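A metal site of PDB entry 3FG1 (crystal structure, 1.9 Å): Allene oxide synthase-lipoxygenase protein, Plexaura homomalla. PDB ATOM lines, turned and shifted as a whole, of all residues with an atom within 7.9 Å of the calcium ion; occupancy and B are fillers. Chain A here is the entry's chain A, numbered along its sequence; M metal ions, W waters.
NH1 of Arg 169 is in salt-bridge range of OD1 of Asp 82. The guanidinium group (NH1) of Arg 169 lies within salt-bridge range of the side-chain carboxylate (OD1) of Asp 84, 2.9 Å away.
Within 4 Å of the calcium ion: His 20, Gly 22, Asp 82 and Asp 84. Along chain A the residues within 4 Å of the calcium ion span positions 20 to 84. The nearest printed residue that does not touch the calcium ion is Ala 21 (4.1 Å).
O of His 20 is bound to the calcium ion, 2.3 Å away. O of Gly 22 is bound to the calcium ion (2.3 Å). The calcium ion is bound by water W1, at 2.4 Å. O of Asp 84 is bound to the calcium ion, 2.4 Å away. O of Asp 82 binds the calcium ion, at 2.4 Å. The calcium ion is bound by OD2 of Asp 82, 2.4 Å away. The calcium ion has six donor atoms within binding distance.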
ATOM      1  N   THR A  15       5.974 -33.556   1.743  1.00  0.00           N
ATOM      2  CA  THR A  15       6.421 -32.206   1.414  1.00  0.00           C
ATOM      3  C   THR A  15       6.884 -32.180  -0.065  1.00  0.00           C
ATOM      4  O   THR A  15       7.560 -33.103  -0.553  1.00  0.00           O
ATOM      5  CB  THR A  15       7.556 -31.786   2.372  1.00  0.00           C
ATOM      6  OG1 THR A  15       7.055 -31.819   3.731  1.00  0.00           O
ATOM      7  CG2 THR A  15       8.143 -30.430   2.025  1.00  0.00           C
ATOM      8  N   ARG A  18      10.063 -29.081  -4.430  1.00  0.00           N
ATOM      9  CA  ARG A  18      10.610 -27.830  -4.981  1.00  0.00           C
ATOM     10  C   ARG A  18      11.492 -27.097  -3.948  1.00  0.00           C
ATOM     11  O   ARG A  18      11.310 -27.240  -2.747  1.00  0.00           O
ATOM     12  CB  ARG A  18       9.509 -26.907  -5.512  1.00  0.00           C
ATOM     13  CG  ARG A  18       8.545 -26.358  -4.430  1.00  0.00           C
ATOM     14  CD  ARG A  18       7.268 -25.749  -5.062  1.00  0.00           C
ATOM     15  NE  ARG A  18       6.473 -26.817  -5.700  1.00  0.00           N
ATOM     16  CZ  ARG A  18       5.389 -26.603  -6.451  1.00  0.00           C
ATOM     17  NH1 ARG A  18       5.001 -25.355  -6.664  1.00  0.00           N
ATOM     18  NH2 ARG A  18       4.713 -27.635  -6.970  1.00  0.00           N
ATOM     19  N   GLU A  19      12.438 -26.312  -4.441  1.00  0.00           N
ATOM     20  CA  GLU A  19      13.313 -25.540  -3.571  1.00  0.00           C
ATOM     21  C   GLU A  19      12.535 -24.757  -2.533  1.00  0.00           C
ATOM     22  O   GLU A  19      11.513 -24.143  -2.841  1.00  0.00           O
ATOM     23  CB  GLU A  19      14.207 -24.596  -4.387  1.00  0.00           C
ATOM     24  CG  GLU A  19      15.390 -25.340  -5.010  1.00  0.00           C
ATOM     25  CD  GLU A  19      16.155 -24.475  -6.003  1.00  0.00           C
ATOM     26  OE1 GLU A  19      16.826 -25.044  -6.886  1.00  0.00           O
ATOM     27  OE2 GLU A  19      16.042 -23.232  -5.911  1.00  0.00           O
ATOM     28  N   HIS A  20      13.035 -24.824  -1.299  1.00  0.00           N
ATOM     29  CA  HIS A  20      12.442 -24.157  -0.131  1.00  0.00           C
ATOM     30  C   HIS A  20      11.112 -24.696   0.310  1.00  0.00           C
ATOM     31  O   HIS A  20      10.472 -24.108   1.183  1.00  0.00           O
ATOM     32  CB  HIS A  20      12.339 -22.663  -0.317  1.00  0.00           C
ATOM     33  CG  HIS A  20      13.654 -21.978  -0.246  1.00  0.00           C
ATOM     34  ND1 HIS A  20      14.583 -22.263   0.738  1.00  0.00           N
ATOM     35  CD2 HIS A  20      14.218 -21.034  -1.037  1.00  0.00           C
ATOM     36  CE1 HIS A  20      15.664 -21.530   0.541  1.00  0.00           C
ATOM     37  NE2 HIS A  20      15.467 -20.767  -0.517  1.00  0.00           N
ATOM     38  N   ALA A  21      10.715 -25.829  -0.267  1.00  0.00           N
ATOM     39  CA  ALA A  21       9.463 -26.492   0.143  1.00  0.00           C
ATOM     40  C   ALA A  21       9.452 -26.828   1.660  1.00  0.00           C
ATOM     41  O   ALA A  21       8.391 -26.856   2.319  1.00  0.00           O
ATOM     42  CB  ALA A  21       9.305 -27.767  -0.652  1.00  0.00           C
ATOM     43  N   GLY A  22      10.638 -27.130   2.189  1.00  0.00           N
ATOM     44  CA  GLY A  22      10.765 -27.651   3.540  1.00  0.00           C
ATOM     45  C   GLY A  22      10.513 -26.598   4.606  1.00  0.00           C
ATOM     46  O   GLY A  22      10.375 -25.381   4.318  1.00  0.00           O
ATOM     47  N   THR A  23      10.504 -27.031   5.869  1.00  0.00           N
ATOM     48  CA  THR A  23      10.331 -26.041   6.920  1.00  0.00           C
ATOM     49  C   THR A  23      10.960 -26.518   8.215  1.00  0.00           C
ATOM     50  O   THR A  23      11.049 -27.727   8.442  1.00  0.00           O
ATOM     51  CB  THR A  23       8.834 -25.728   7.159  1.00  0.00           C
ATOM     52  OG1 THR A  23       8.716 -24.620   8.042  1.00  0.00           O
ATOM     53  CG2 THR A  23       8.087 -26.932   7.754  1.00  0.00           C
ATOM     54  N   ASP A  24      11.410 -25.569   9.037  1.00  0.00           N
ATOM     55  CA  ASP A  24      11.741 -25.911  10.429  1.00  0.00           C
ATOM     56  C   ASP A  24      10.840 -25.245  11.473  1.00  0.00           C
ATOM     57  O   ASP A  24      11.173 -25.201  12.658  1.00  0.00           O
ATOM     58  CB  ASP A  24      13.232 -25.706  10.716  1.00  0.00           C
ATOM     59  CG  ASP A  24      13.634 -24.257  10.790  1.00  0.00           C
ATOM     60  OD1 ASP A  24      12.787 -23.352  10.675  1.00  0.00           O
ATOM     61  OD2 ASP A  24      14.838 -24.011  10.990  1.00  0.00           O
ATOM     62  N   ALA A  25       9.698 -24.748  11.012  1.00  0.00           N
ATOM     63  CA  ALA A  25       8.696 -24.221  11.904  1.00  0.00           C
ATOM     64  C   ALA A  25       8.128 -25.364  12.708  1.00  0.00           C
ATOM     65  O   ALA A  25       8.226 -26.547  12.311  1.00  0.00           O
ATOM     66  CB  ALA A  25       7.594 -23.547  11.110  1.00  0.00           C
ATOM     67  N   PHE A  48      11.260 -31.695   8.271  1.00  0.00           N
ATOM     68  CA  PHE A  48      10.409 -31.626   7.102  1.00  0.00           C
ATOM     69  C   PHE A  48      11.280 -31.086   5.933  1.00  0.00           C
ATOM     70  O   PHE A  48      11.242 -29.895   5.608  1.00  0.00           O
ATOM     71  CB  PHE A  48       9.217 -30.667   7.349  1.00  0.00           C
ATOM     72  CG  PHE A  48       8.080 -31.296   8.140  1.00  0.00           C
ATOM     73  CD1 PHE A  48       7.646 -30.693   9.315  1.00  0.00           C
ATOM     74  CD2 PHE A  48       7.459 -32.476   7.693  1.00  0.00           C
ATOM     75  CE1 PHE A  48       6.592 -31.248  10.041  1.00  0.00           C
ATOM     76  CE2 PHE A  48       6.385 -33.050   8.430  1.00  0.00           C
ATOM     77  CZ  PHE A  48       5.981 -32.417   9.603  1.00  0.00           C
ATOM     78  N   GLY A  81      15.167 -19.743   8.330  1.00  0.00           N
ATOM     79  CA  GLY A  81      15.432 -19.055   7.062  1.00  0.00           C
ATOM     80  C   GLY A  81      14.188 -18.874   6.210  1.00  0.00           C
ATOM     81  O   GLY A  81      13.891 -17.755   5.757  1.00  0.00           O
ATOM     82  N   ASP A  82      13.446 -19.964   5.996  1.00  0.00           N
ATOM     83  CA  ASP A  82      12.241 -19.884   5.142  1.00  0.00           C
ATOM     84  C   ASP A  82      11.160 -20.822   5.694  1.00  0.00           C
ATOM     85  O   ASP A  82      11.041 -21.935   5.229  1.00  0.00           O
ATOM     86  CB  ASP A  82      12.605 -20.215   3.686  1.00  0.00           C
ATOM     87  CG  ASP A  82      11.422 -20.092   2.739  1.00  0.00           C
ATOM     88  OD1 ASP A  82      11.063 -18.955   2.384  1.00  0.00           O
ATOM     89  OD2 ASP A  82      10.854 -21.139   2.334  1.00  0.00           O
ATOM     90  N   PRO A  83      10.405 -20.372   6.715  1.00  0.00           N
ATOM     91  CA  PRO A  83       9.386 -21.184   7.370  1.00  0.00           C
ATOM     92  C   PRO A  83       8.228 -21.660   6.475  1.00  0.00           C
ATOM     93  O   PRO A  83       7.609 -22.696   6.780  1.00  0.00           O
ATOM     94  CB  PRO A  83       8.869 -20.270   8.502  1.00  0.00           C
ATOM     95  CG  PRO A  83       9.259 -18.855   8.077  1.00  0.00           C
ATOM     96  CD  PRO A  83      10.585 -19.066   7.388  1.00  0.00           C
ATOM     97  N   ASP A  84       7.941 -20.936   5.388  1.00  0.00           N
ATOM     98  CA  ASP A  84       6.854 -21.354   4.490  1.00  0.00           C
ATOM     99  C   ASP A  84       7.109 -22.777   4.002  1.00  0.00           C
ATOM    100  O   ASP A  84       8.235 -23.176   3.704  1.00  0.00           O
ATOM    101  CB  ASP A  84       6.674 -20.439   3.301  1.00  0.00           C
ATOM    102  CG  ASP A  84       6.230 -19.040   3.658  1.00  0.00           C
ATOM    103  OD1 ASP A  84       6.264 -18.225   2.699  1.00  0.00           O
ATOM    104  OD2 ASP A  84       5.830 -18.719   4.823  1.00  0.00           O
ATOM    105  N   TRP A  85       6.052 -23.550   3.911  1.00  0.00           N
ATOM    106  CA  TRP A  85       6.141 -25.005   3.783  1.00  0.00           C
ATOM    107  C   TRP A  85       5.237 -25.455   2.630  1.00  0.00           C
ATOM    108  O   TRP A  85       4.041 -25.232   2.688  1.00  0.00           O
ATOM    109  CB  TRP A  85       5.647 -25.603   5.102  1.00  0.00           C
ATOM    110  CG  TRP A  85       5.660 -27.108   5.237  1.00  0.00           C
ATOM    111  CD1 TRP A  85       6.539 -27.983   4.649  1.00  0.00           C
ATOM    112  CD2 TRP A  85       4.828 -27.890   6.103  1.00  0.00           C
ATOM    113  NE1 TRP A  85       6.262 -29.301   5.058  1.00  0.00           N
ATOM    114  CE2 TRP A  85       5.229 -29.264   5.954  1.00  0.00           C
ATOM    115  CE3 TRP A  85       3.762 -27.584   6.969  1.00  0.00           C
ATOM    116  CZ2 TRP A  85       4.614 -30.302   6.670  1.00  0.00           C
ATOM    117  CZ3 TRP A  85       3.117 -28.644   7.646  1.00  0.00           C
ATOM    118  CH2 TRP A  85       3.549 -29.979   7.495  1.00  0.00           C
ATOM    119  N   PHE A  86       5.799 -26.062   1.597  1.00  0.00           N
ATOM    120  CA  PHE A  86       4.966 -26.480   0.482  1.00  0.00           C
ATOM    121  C   PHE A  86       4.569 -27.940   0.699  1.00  0.00           C
ATOM    122  O   PHE A  86       5.410 -28.838   0.623  1.00  0.00           O
ATOM    123  CB  PHE A  86       5.680 -26.341  -0.871  1.00  0.00           C
ATOM    124  CG  PHE A  86       4.762 -26.582  -2.050  1.00  0.00           C
ATOM    125  CD1 PHE A  86       4.116 -25.506  -2.665  1.00  0.00           C
ATOM    126  CD2 PHE A  86       4.469 -27.868  -2.475  1.00  0.00           C
ATOM    127  CE1 PHE A  86       3.217 -25.729  -3.735  1.00  0.00           C
ATOM    128  CE2 PHE A  86       3.580 -28.091  -3.544  1.00  0.00           C
ATOM    129  CZ  PHE A  86       2.963 -27.027  -4.169  1.00  0.00           C
ATOM    130  N   TRP A 108       1.219 -23.626  -0.721  1.00  0.00           N
ATOM    131  CA  TRP A 108       2.103 -23.201   0.354  1.00  0.00           C
ATOM    132  C   TRP A 108       1.376 -23.021   1.685  1.00  0.00           C
ATOM    133  O   TRP A 108       0.340 -22.360   1.745  1.00  0.00           O
ATOM    134  CB  TRP A 108       2.809 -21.901  -0.018  1.00  0.00           C
ATOM    135  CG  TRP A 108       3.849 -22.128  -1.051  1.00  0.00           C
ATOM    136  CD1 TRP A 108       3.682 -22.028  -2.403  1.00  0.00           C
ATOM    137  CD2 TRP A 108       5.218 -22.507  -0.835  1.00  0.00           C
ATOM    138  NE1 TRP A 108       4.866 -22.313  -3.059  1.00  0.00           N
ATOM    139  CE2 TRP A 108       5.836 -22.592  -2.124  1.00  0.00           C
ATOM    140  CE3 TRP A 108       6.005 -22.768   0.307  1.00  0.00           C
ATOM    141  CZ2 TRP A 108       7.190 -22.957  -2.291  1.00  0.00           C
ATOM    142  CZ3 TRP A 108       7.370 -23.123   0.139  1.00  0.00           C
ATOM    143  CH2 TRP A 108       7.937 -23.216  -1.150  1.00  0.00           C
ATOM    144  N   VAL A 109       1.978 -23.553   2.753  1.00  0.00           N
ATOM    145  CA  VAL A 109       1.482 -23.377   4.097  1.00  0.00           C
ATOM    146  C   VAL A 109       2.268 -22.246   4.771  1.00  0.00           C
ATOM    147  O   VAL A 109       3.494 -22.334   4.944  1.00  0.00           O
ATOM    148  CB  VAL A 109       1.549 -24.684   4.932  1.00  0.00           C
ATOM    149  CG1 VAL A 109       1.072 -24.441   6.392  1.00  0.00           C
ATOM    150  CG2 VAL A 109       0.734 -25.777   4.215  1.00  0.00           C
ATOM    151  N   ARG A 169       2.460 -16.474  -2.408  1.00  0.00           N
ATOM    152  CA  ARG A 169       3.494 -17.439  -2.807  1.00  0.00           C
ATOM    153  C   ARG A 169       2.994 -18.508  -3.782  1.00  0.00           C
ATOM    154  O   ARG A 169       3.785 -19.014  -4.588  1.00  0.00           O
ATOM    155  CB  ARG A 169       4.171 -18.093  -1.599  1.00  0.00           C
ATOM    156  CG  ARG A 169       5.586 -18.551  -1.929  1.00  0.00           C
ATOM    157  CD  ARG A 169       6.338 -18.964  -0.677  1.00  0.00           C
ATOM    158  NE  ARG A 169       7.640 -19.548  -0.989  1.00  0.00           N
ATOM    159  CZ  ARG A 169       8.688 -19.535  -0.154  1.00  0.00           C
ATOM    160  NH1 ARG A 169       8.583 -18.949   1.037  1.00  0.00           N
ATOM    161  NH2 ARG A 169       9.851 -20.090  -0.520  1.00  0.00           N
HETATM  162 CA    CA M   1      10.559 -23.258   3.340  1.00  0.00          CA
HETATM  163  O   HOH W   1      12.859 -23.746   3.315  1.00  0.00           O
